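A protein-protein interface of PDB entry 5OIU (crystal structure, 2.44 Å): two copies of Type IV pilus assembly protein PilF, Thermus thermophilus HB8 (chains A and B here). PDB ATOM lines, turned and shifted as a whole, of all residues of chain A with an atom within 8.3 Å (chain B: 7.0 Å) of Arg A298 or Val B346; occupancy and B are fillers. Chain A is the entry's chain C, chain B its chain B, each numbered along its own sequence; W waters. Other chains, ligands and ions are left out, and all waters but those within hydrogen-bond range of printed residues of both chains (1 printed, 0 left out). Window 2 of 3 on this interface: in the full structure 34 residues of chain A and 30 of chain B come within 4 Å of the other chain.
ND1 of His B343 lies within hydrogen-bond range of OD2 of Asp A292 (2.8 Å). The backbone carbonyl oxygen (O) of Val B346 sits close to the guanidinium group (NH2) of Arg A298.
OD1 of Asp A292 lies close to N of Glu A294 (3.3 Å). The side-chain carboxylate of Glu A294 is in salt-bridge range of the guanidinium group of Arg A297.
Asp A292 touches Val B346. Glu A294 touches His B343 (CG to CE1, 3.9 Å). CG2 of Val B346 touches CB of Glu A294, 3.8 Å away. OG1 of Thr A295 touches CG1 of Val B346 (3.9 Å). CG of Pro B262 touches NH1 of Arg A298, 3.4 Å away. Phe B263 touches Leu A299. Arg A367 touches Phe B263 (NH1 to CZ, 3.6 Å). NH2 of Arg A367 touches ND2 of Asn B264, at 3.99 Å.
Arg A298 touches two residues of chain B. Val B346 touches just these residues of chain A: Asp A292 (3.3 Å), Glu A294 (3.8 Å), Thr A295 (3.9 Å) and Arg A298 (2.2 Å). No residue of chain A comes within 4 Å of Ala B347. Of the printed residues of chain B, Arg A367 touches Phe B263 and Asn B264. Printed residues of chain B within 4 Å of Asp A292: His B343 and Val B346. The nearest residue of chain B that does not touch Arg A298 is Ile B345 (4.05 Å).
Of the 15 printed residues of chain A, 6 touch a printed residue of chain B. Hydrophobic or aromatic side chains of chain A that line the printed part of chain B: Leu A299. Of the 17 printed residues of chain B, 5 touch a printed residue of chain A. Among the printed residues, 10 pairs touch across the chains. Among the printed residues, no Asp or Glu carboxylate lies within 4 Å of a Lys or Arg side-chain nitrogen of the other chain.
No position is printed for both chains.
Water W1 bridges OD1 of Asn B264 and NH2 of Arg A367.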
ATOM      1  N   ASP A 292       4.117   8.873  15.840  1.00  0.00           N
ATOM      2  CA  ASP A 292       5.129   8.167  15.062  1.00  0.00           C
ATOM      3  C   ASP A 292       4.968   8.522  13.589  1.00  0.00           C
ATOM      4  O   ASP A 292       3.896   8.270  13.015  1.00  0.00           O
ATOM      5  CB  ASP A 292       5.000   6.659  15.252  1.00  0.00           C
ATOM      6  CG  ASP A 292       6.242   5.894  14.792  1.00  0.00           C
ATOM      7  OD1 ASP A 292       7.118   6.518  14.152  1.00  0.00           O
ATOM      8  OD2 ASP A 292       6.346   4.671  15.082  1.00  0.00           O
ATOM      9  N   PRO A 293       5.983   9.093  12.939  1.00  0.00           N
ATOM     10  CA  PRO A 293       5.880   9.327  11.487  1.00  0.00           C
ATOM     11  C   PRO A 293       5.461   8.096  10.702  1.00  0.00           C
ATOM     12  O   PRO A 293       4.677   8.222   9.758  1.00  0.00           O
ATOM     13  CB  PRO A 293       7.294   9.775  11.107  1.00  0.00           C
ATOM     14  CG  PRO A 293       7.847  10.341  12.344  1.00  0.00           C
ATOM     15  CD  PRO A 293       7.262   9.564  13.489  1.00  0.00           C
ATOM     16  N   GLU A 294       5.946   6.907  11.070  1.00  0.00           N
ATOM     17  CA  GLU A 294       5.597   5.709  10.314  1.00  0.00           C
ATOM     18  C   GLU A 294       4.100   5.435  10.358  1.00  0.00           C
ATOM     19  O   GLU A 294       3.497   5.127   9.325  1.00  0.00           O
ATOM     20  CB  GLU A 294       6.374   4.509  10.840  1.00  0.00           C
ATOM     21  CG  GLU A 294       7.783   4.428  10.322  1.00  0.00           C
ATOM     22  CD  GLU A 294       7.870   3.960   8.871  1.00  0.00           C
ATOM     23  OE1 GLU A 294       6.857   4.029   8.119  1.00  0.00           O
ATOM     24  OE2 GLU A 294       8.977   3.521   8.485  1.00  0.00           O
ATOM     25  N   THR A 295       3.484   5.550  11.545  1.00  0.00           N
ATOM     26  CA  THR A 295       2.034   5.385  11.661  1.00  0.00           C
ATOM     27  C   THR A 295       1.304   6.258  10.651  1.00  0.00           C
ATOM     28  O   THR A 295       0.469   5.773   9.882  1.00  0.00           O
ATOM     29  CB  THR A 295       1.539   5.739  13.069  1.00  0.00           C
ATOM     30  OG1 THR A 295       2.332   5.102  14.073  1.00  0.00           O
ATOM     31  CG2 THR A 295       0.101   5.312  13.219  1.00  0.00           C
ATOM     32  N   LEU A 296       1.607   7.565  10.659  1.00  0.00           N
ATOM     33  CA  LEU A 296       0.976   8.503   9.728  1.00  0.00           C
ATOM     34  C   LEU A 296       1.259   8.132   8.279  1.00  0.00           C
ATOM     35  O   LEU A 296       0.375   8.235   7.420  1.00  0.00           O
ATOM     36  CB  LEU A 296       1.459   9.927  10.010  1.00  0.00           C
ATOM     37  CG  LEU A 296       1.169  10.452  11.413  1.00  0.00           C
ATOM     38  CD1 LEU A 296       1.784  11.826  11.569  1.00  0.00           C
ATOM     39  CD2 LEU A 296      -0.339  10.497  11.671  1.00  0.00           C
ATOM     40  N   ARG A 297       2.496   7.719   7.989  1.00  0.00           N
ATOM     41  CA  ARG A 297       2.851   7.261   6.651  1.00  0.00           C
ATOM     42  C   ARG A 297       1.944   6.115   6.221  1.00  0.00           C
ATOM     43  O   ARG A 297       1.265   6.197   5.190  1.00  0.00           O
ATOM     44  CB  ARG A 297       4.321   6.833   6.629  1.00  0.00           C
ATOM     45  CG  ARG A 297       5.188   7.511   5.593  1.00  0.00           C
ATOM     46  CD  ARG A 297       6.648   7.095   5.736  1.00  0.00           C
ATOM     47  NE  ARG A 297       7.480   8.159   6.306  1.00  0.00           N
ATOM     48  CZ  ARG A 297       8.080   8.098   7.496  1.00  0.00           C
ATOM     49  NH1 ARG A 297       7.938   7.025   8.264  1.00  0.00           N
ATOM     50  NH2 ARG A 297       8.823   9.110   7.928  1.00  0.00           N
ATOM     51  N   ARG A 298       1.896   5.040   7.019  1.00  0.00           N
ATOM     52  CA  ARG A 298       1.062   3.904   6.638  1.00  0.00           C
ATOM     53  C   ARG A 298      -0.420   4.257   6.638  1.00  0.00           C
ATOM     54  O   ARG A 298      -1.212   3.547   6.010  1.00  0.00           O
ATOM     55  CB  ARG A 298       1.317   2.683   7.533  1.00  0.00           C
ATOM     56  CG  ARG A 298       2.725   2.582   8.121  1.00  0.00           C
ATOM     57  CD  ARG A 298       3.703   1.713   7.288  1.00  0.00           C
ATOM     58  NE  ARG A 298       3.161   0.386   6.993  1.00  0.00           N
ATOM     59  CZ  ARG A 298       3.120  -0.618   7.867  1.00  0.00           C
ATOM     60  NH1 ARG A 298       2.606  -1.789   7.509  1.00  0.00           N
ATOM     61  NH2 ARG A 298       3.580  -0.447   9.097  1.00  0.00           N
ATOM     62  N   LEU A 299      -0.815   5.357   7.279  1.00  0.00           N
ATOM     63  CA  LEU A 299      -2.175   5.861   7.159  1.00  0.00           C
ATOM     64  C   LEU A 299      -2.344   6.760   5.938  1.00  0.00           C
ATOM     65  O   LEU A 299      -3.336   7.489   5.836  1.00  0.00           O
ATOM     66  CB  LEU A 299      -2.586   6.590   8.440  1.00  0.00           C
ATOM     67  CG  LEU A 299      -2.770   5.646   9.638  1.00  0.00           C
ATOM     68  CD1 LEU A 299      -2.656   6.362  10.977  1.00  0.00           C
ATOM     69  CD2 LEU A 299      -4.097   4.912   9.536  1.00  0.00           C
ATOM     70  N   GLY A 300      -1.386   6.727   5.013  1.00  0.00           N
ATOM     71  CA  GLY A 300      -1.546   7.413   3.750  1.00  0.00           C
ATOM     72  C   GLY A 300      -1.411   8.909   3.818  1.00  0.00           C
ATOM     73  O   GLY A 300      -1.949   9.608   2.952  1.00  0.00           O
ATOM     74  N   LEU A 301      -0.706   9.424   4.823  1.00  0.00           N
ATOM     75  CA  LEU A 301      -0.466  10.852   4.964  1.00  0.00           C
ATOM     76  C   LEU A 301       0.809  11.259   4.224  1.00  0.00           C
ATOM     77  O   LEU A 301       1.825  10.555   4.270  1.00  0.00           O
ATOM     78  CB  LEU A 301      -0.364  11.216   6.443  1.00  0.00           C
ATOM     79  CG  LEU A 301      -0.632  12.667   6.807  1.00  0.00           C
ATOM     80  CD1 LEU A 301      -2.049  13.001   6.444  1.00  0.00           C
ATOM     81  CD2 LEU A 301      -0.387  12.891   8.281  1.00  0.00           C
ATOM     82  N   SER A 302       0.745  12.398   3.535  1.00  0.00           N
ATOM     83  CA  SER A 302       1.884  12.887   2.766  1.00  0.00           C
ATOM     84  C   SER A 302       3.010  13.315   3.693  1.00  0.00           C
ATOM     85  O   SER A 302       2.776  13.769   4.816  1.00  0.00           O
ATOM     86  CB  SER A 302       1.477  14.076   1.902  1.00  0.00           C
ATOM     87  OG  SER A 302       1.316  15.229   2.714  1.00  0.00           O
ATOM     88  N   GLU A 303       4.248  13.189   3.206  1.00  0.00           N
ATOM     89  CA  GLU A 303       5.378  13.490   4.079  1.00  0.00           C
ATOM     90  C   GLU A 303       5.441  14.969   4.418  1.00  0.00           C
ATOM     91  O   GLU A 303       5.919  15.337   5.500  1.00  0.00           O
ATOM     92  CB  GLU A 303       6.695  13.031   3.451  1.00  0.00           C
ATOM     93  CG  GLU A 303       7.708  12.585   4.492  1.00  0.00           C
ATOM     94  CD  GLU A 303       7.586  11.106   4.819  1.00  0.00           C
ATOM     95  OE1 GLU A 303       6.789  10.390   4.164  1.00  0.00           O
ATOM     96  OE2 GLU A 303       8.271  10.654   5.758  1.00  0.00           O
ATOM     97  N   ILE A 306       3.095  15.190   7.274  1.00  0.00           N
ATOM     98  CA  ILE A 306       3.645  14.619   8.503  1.00  0.00           C
ATOM     99  C   ILE A 306       4.446  15.668   9.270  1.00  0.00           C
ATOM    100  O   ILE A 306       4.393  15.718  10.505  1.00  0.00           O
ATOM    101  CB  ILE A 306       4.492  13.367   8.189  1.00  0.00           C
ATOM    102  CG1 ILE A 306       3.589  12.216   7.748  1.00  0.00           C
ATOM    103  CG2 ILE A 306       5.319  12.943   9.402  1.00  0.00           C
ATOM    104  CD1 ILE A 306       4.340  11.022   7.213  1.00  0.00           C
ATOM    105  N   ARG A 367     -11.566   6.492   7.695  1.00  0.00           N
ATOM    106  CA  ARG A 367     -10.337   6.554   8.472  1.00  0.00           C
ATOM    107  C   ARG A 367      -9.513   7.775   8.091  1.00  0.00           C
ATOM    108  O   ARG A 367      -8.900   8.419   8.956  1.00  0.00           O
ATOM    109  CB  ARG A 367      -9.547   5.270   8.274  1.00  0.00           C
ATOM    110  CG  ARG A 367      -8.279   5.191   9.077  1.00  0.00           C
ATOM    111  CD  ARG A 367      -7.501   3.984   8.632  1.00  0.00           C
ATOM    112  NE  ARG A 367      -7.893   2.784   9.354  1.00  0.00           N
ATOM    113  CZ  ARG A 367      -7.857   1.556   8.839  1.00  0.00           C
ATOM    114  NH1 ARG A 367      -7.457   1.368   7.577  1.00  0.00           N
ATOM    115  NH2 ARG A 367      -8.219   0.517   9.591  1.00  0.00           N
ATOM    116  N   LEU A 371      -8.780  10.507  10.701  1.00  0.00           N
ATOM    117  CA  LEU A 371      -7.418  10.939  10.994  1.00  0.00           C
ATOM    118  C   LEU A 371      -7.319  12.456  10.949  1.00  0.00           C
ATOM    119  O   LEU A 371      -6.776  13.088  11.863  1.00  0.00           O
ATOM    120  CB  LEU A 371      -6.431  10.304  10.013  1.00  0.00           C
ATOM    121  CG  LEU A 371      -5.009  10.838  10.198  1.00  0.00           C
ATOM    122  CD1 LEU A 371      -4.506  10.475  11.574  1.00  0.00           C
ATOM    123  CD2 LEU A 371      -4.043  10.352   9.134  1.00  0.00           C
ATOM    124  N   ASP B 256      -0.694  -9.627  12.162  1.00  0.00           N
ATOM    125  CA  ASP B 256      -0.556  -9.066  10.822  1.00  0.00           C
ATOM    126  C   ASP B 256      -1.052 -10.051   9.764  1.00  0.00           C
ATOM    127  O   ASP B 256      -1.894  -9.703   8.924  1.00  0.00           O
ATOM    128  CB  ASP B 256       0.898  -8.662  10.552  1.00  0.00           C
ATOM    129  CG  ASP B 256       1.062  -7.815   9.270  1.00  0.00           C
ATOM    130  OD1 ASP B 256       0.056  -7.516   8.574  1.00  0.00           O
ATOM    131  OD2 ASP B 256       2.219  -7.450   8.959  1.00  0.00           O
ATOM    132  N   GLU B 261      -4.076  -4.664  10.726  1.00  0.00           N
ATOM    133  CA  GLU B 261      -3.084  -3.736  10.204  1.00  0.00           C
ATOM    134  C   GLU B 261      -2.069  -3.395  11.295  1.00  0.00           C
ATOM    135  O   GLU B 261      -2.444  -3.236  12.460  1.00  0.00           O
ATOM    136  CB  GLU B 261      -3.765  -2.466   9.692  1.00  0.00           C
ATOM    137  CG  GLU B 261      -4.604  -2.672   8.427  1.00  0.00           C
ATOM    138  CD  GLU B 261      -3.770  -2.922   7.169  1.00  0.00           C
ATOM    139  OE1 GLU B 261      -4.210  -3.735   6.317  1.00  0.00           O
ATOM    140  OE2 GLU B 261      -2.686  -2.304   7.019  1.00  0.00           O
ATOM    141  N   PRO B 262      -0.783  -3.309  10.965  1.00  0.00           N
ATOM    142  CA  PRO B 262       0.224  -3.017  12.000  1.00  0.00           C
ATOM    143  C   PRO B 262      -0.079  -1.790  12.823  1.00  0.00           C
ATOM    144  O   PRO B 262       0.282  -1.763  14.012  1.00  0.00           O
ATOM    145  CB  PRO B 262       1.510  -2.832  11.192  1.00  0.00           C
ATOM    146  CG  PRO B 262       1.298  -3.729   9.992  1.00  0.00           C
ATOM    147  CD  PRO B 262      -0.176  -3.708   9.684  1.00  0.00           C
ATOM    148  N   PHE B 263      -0.727  -0.759  12.250  1.00  0.00           N
ATOM    149  CA  PHE B 263      -0.987   0.419  13.077  1.00  0.00           C
ATOM    150  C   PHE B 263      -2.047   0.118  14.129  1.00  0.00           C
ATOM    151  O   PHE B 263      -2.060   0.748  15.193  1.00  0.00           O
ATOM    152  CB  PHE B 263      -1.360   1.649  12.236  1.00  0.00           C
ATOM    153  CG  PHE B 263      -2.393   1.397  11.153  1.00  0.00           C
ATOM    154  CD1 PHE B 263      -3.746   1.286  11.464  1.00  0.00           C
ATOM    155  CD2 PHE B 263      -2.015   1.333   9.824  1.00  0.00           C
ATOM    156  CE1 PHE B 263      -4.688   1.079  10.464  1.00  0.00           C
ATOM    157  CE2 PHE B 263      -2.949   1.120   8.822  1.00  0.00           C
ATOM    158  CZ  PHE B 263      -4.288   0.992   9.138  1.00  0.00           C
ATOM    159  N   ASN B 264      -2.894  -0.881  13.879  1.00  0.00           N
ATOM    160  CA  ASN B 264      -3.863  -1.321  14.880  1.00  0.00           C
ATOM    161  C   ASN B 264      -3.196  -2.156  15.976  1.00  0.00           C
ATOM    162  O   ASN B 264      -3.409  -1.911  17.171  1.00  0.00           O
ATOM    163  CB  ASN B 264      -4.997  -2.091  14.190  1.00  0.00           C
ATOM    164  CG  ASN B 264      -5.905  -1.181  13.386  1.00  0.00           C
ATOM    165  OD1 ASN B 264      -5.915   0.047  13.595  1.00  0.00           O
ATOM    166  ND2 ASN B 264      -6.696  -1.769  12.481  1.00  0.00           N
ATOM    167  N   ILE B 265      -2.378  -3.140  15.585  1.00  0.00           N
ATOM    168  CA  ILE B 265      -1.533  -3.870  16.531  1.00  0.00           C
ATOM    169  C   ILE B 265      -0.763  -2.904  17.418  1.00  0.00           C
ATOM    170  O   ILE B 265      -0.778  -3.000  18.649  1.00  0.00           O
ATOM    171  CB  ILE B 265      -0.547  -4.778  15.781  1.00  0.00           C
ATOM    172  CG1 ILE B 265      -1.268  -5.652  14.761  1.00  0.00           C
ATOM    173  CG2 ILE B 265       0.299  -5.569  16.791  1.00  0.00           C
ATOM    174  CD1 ILE B 265      -0.336  -6.471  13.921  1.00  0.00           C
ATOM    175  N   SER B 266      -0.033  -1.991  16.781  1.00  0.00           N
ATOM    176  CA  SER B 266       0.823  -1.052  17.492  1.00  0.00           C
ATOM    177  C   SER B 266       0.050  -0.244  18.531  1.00  0.00           C
ATOM    178  O   SER B 266       0.572   0.061  19.613  1.00  0.00           O
ATOM    179  CB  SER B 266       1.480  -0.122  16.475  1.00  0.00           C
ATOM    180  OG  SER B 266       2.461   0.659  17.097  1.00  0.00           O
ATOM    181  N   ALA B 267      -1.196   0.118  18.220  1.00  0.00           N
ATOM    182  CA  ALA B 267      -1.999   0.892  19.155  1.00  0.00           C
ATOM    183  C   ALA B 267      -2.688   0.030  20.198  1.00  0.00           C
ATOM    184  O   ALA B 267      -3.085   0.544  21.248  1.00  0.00           O
ATOM    185  CB  ALA B 267      -3.052   1.698  18.399  1.00  0.00           C
ATOM    186  N   ILE B 341       9.280  -0.982  20.508  1.00  0.00           N
ATOM    187  CA  ILE B 341       8.625  -2.108  19.855  1.00  0.00           C
ATOM    188  C   ILE B 341       7.456  -1.629  19.000  1.00  0.00           C
ATOM    189  O   ILE B 341       7.255  -2.100  17.865  1.00  0.00           O
ATOM    190  CB  ILE B 341       8.183  -3.139  20.905  1.00  0.00           C
ATOM    191  CG1 ILE B 341       9.398  -3.592  21.707  1.00  0.00           C
ATOM    192  CG2 ILE B 341       7.510  -4.317  20.243  1.00  0.00           C
ATOM    193  CD1 ILE B 341       9.260  -4.965  22.263  1.00  0.00           C
ATOM    194  N   ARG B 342       6.665  -0.692  19.532  1.00  0.00           N
ATOM    195  CA  ARG B 342       5.600  -0.086  18.741  1.00  0.00           C
ATOM    196  C   ARG B 342       6.137   0.456  17.416  1.00  0.00           C
ATOM    197  O   ARG B 342       5.492   0.310  16.365  1.00  0.00           O
ATOM    198  CB  ARG B 342       4.908   1.024  19.543  1.00  0.00           C
ATOM    199  CG  ARG B 342       3.738   0.538  20.380  1.00  0.00           C
ATOM    200  CD  ARG B 342       2.980   1.693  21.003  1.00  0.00           C
ATOM    201  NE  ARG B 342       3.733   2.273  22.103  1.00  0.00           N
ATOM    202  CZ  ARG B 342       3.639   1.843  23.354  1.00  0.00           C
ATOM    203  NH1 ARG B 342       2.806   0.844  23.638  1.00  0.00           N
ATOM    204  NH2 ARG B 342       4.376   2.402  24.308  1.00  0.00           N
ATOM    205  N   HIS B 343       7.332   1.058  17.433  1.00  0.00           N
ATOM    206  CA  HIS B 343       7.882   1.550  16.176  1.00  0.00           C
ATOM    207  C   HIS B 343       8.254   0.398  15.261  1.00  0.00           C
ATOM    208  O   HIS B 343       7.975   0.438  14.058  1.00  0.00           O
ATOM    209  CB  HIS B 343       9.092   2.440  16.419  1.00  0.00           C
ATOM    210  CG  HIS B 343       9.552   3.146  15.184  1.00  0.00           C
ATOM    211  ND1 HIS B 343       9.096   4.398  14.829  1.00  0.00           N
ATOM    212  CD2 HIS B 343      10.392   2.759  14.195  1.00  0.00           C
ATOM    213  CE1 HIS B 343       9.653   4.760  13.686  1.00  0.00           C
ATOM    214  NE2 HIS B 343      10.443   3.783  13.280  1.00  0.00           N
ATOM    215  N   ALA B 344       8.863  -0.647  15.821  1.00  0.00           N
ATOM    216  CA  ALA B 344       9.261  -1.794  15.022  1.00  0.00           C
ATOM    217  C   ALA B 344       8.066  -2.409  14.308  1.00  0.00           C
ATOM    218  O   ALA B 344       8.182  -2.878  13.165  1.00  0.00           O
ATOM    219  CB  ALA B 344       9.951  -2.829  15.909  1.00  0.00           C
ATOM    220  N   ILE B 345       6.909  -2.425  14.964  1.00  0.00           N
ATOM    221  CA  ILE B 345       5.731  -3.027  14.351  1.00  0.00           C
ATOM    222  C   ILE B 345       5.292  -2.213  13.137  1.00  0.00           C
ATOM    223  O   ILE B 345       5.118  -2.760  12.043  1.00  0.00           O
ATOM    224  CB  ILE B 345       4.608  -3.171  15.392  1.00  0.00           C
ATOM    225  CG1 ILE B 345       5.069  -4.079  16.534  1.00  0.00           C
ATOM    226  CG2 ILE B 345       3.338  -3.674  14.762  1.00  0.00           C
ATOM    227  CD1 ILE B 345       4.245  -3.957  17.805  1.00  0.00           C
ATOM    228  N   VAL B 346       5.145  -0.887  13.299  1.00  0.00           N
ATOM    229  CA  VAL B 346       4.704  -0.050  12.175  1.00  0.00           C
ATOM    230  C   VAL B 346       5.786   0.067  11.117  1.00  0.00           C
ATOM    231  O   VAL B 346       5.487   0.330   9.948  1.00  0.00           O
ATOM    232  CB  VAL B 346       4.262   1.360  12.624  1.00  0.00           C
ATOM    233  CG1 VAL B 346       2.886   1.319  13.241  1.00  0.00           C
ATOM    234  CG2 VAL B 346       5.291   1.997  13.548  1.00  0.00           C
ATOM    235  N   ALA B 347       7.046  -0.087  11.491  1.00  0.00           N
ATOM    236  CA  ALA B 347       8.057  -0.127  10.448  1.00  0.00           C
ATOM    237  C   ALA B 347       8.106  -1.472   9.744  1.00  0.00           C
ATOM    238  O   ALA B 347       8.959  -1.657   8.871  1.00  0.00           O
ATOM    239  CB  ALA B 347       9.432   0.218  11.023  1.00  0.00           C
ATOM    240  N   GLY B 348       7.233  -2.412  10.109  1.00  0.00           N
ATOM    241  CA  GLY B 348       7.143  -3.697   9.437  1.00  0.00           C
ATOM    242  C   GLY B 348       8.276  -4.672   9.703  1.00  0.00           C
ATOM    243  O   GLY B 348       8.553  -5.517   8.851  1.00  0.00           O
ATOM    244  N   LYS B 349       8.935  -4.595  10.859  1.00  0.00           N
ATOM    245  CA  LYS B 349      10.042  -5.504  11.112  1.00  0.00           C
ATOM    246  C   LYS B 349       9.540  -6.915  11.404  1.00  0.00           C
ATOM    247  O   LYS B 349       8.411  -7.126  11.867  1.00  0.00           O
ATOM    248  CB  LYS B 349      10.907  -5.000  12.258  1.00  0.00           C
ATOM    249  CG  LYS B 349      11.279  -3.546  12.094  1.00  0.00           C
ATOM    250  CD  LYS B 349      12.756  -3.324  12.258  1.00  0.00           C
ATOM    251  CE  LYS B 349      13.178  -2.025  11.600  1.00  0.00           C
ATOM    252  NZ  LYS B 349      13.248  -2.172  10.120  1.00  0.00           N
HETATM  253  O   HOH W   1      -8.391   0.614  12.475  1.00  0.00           O
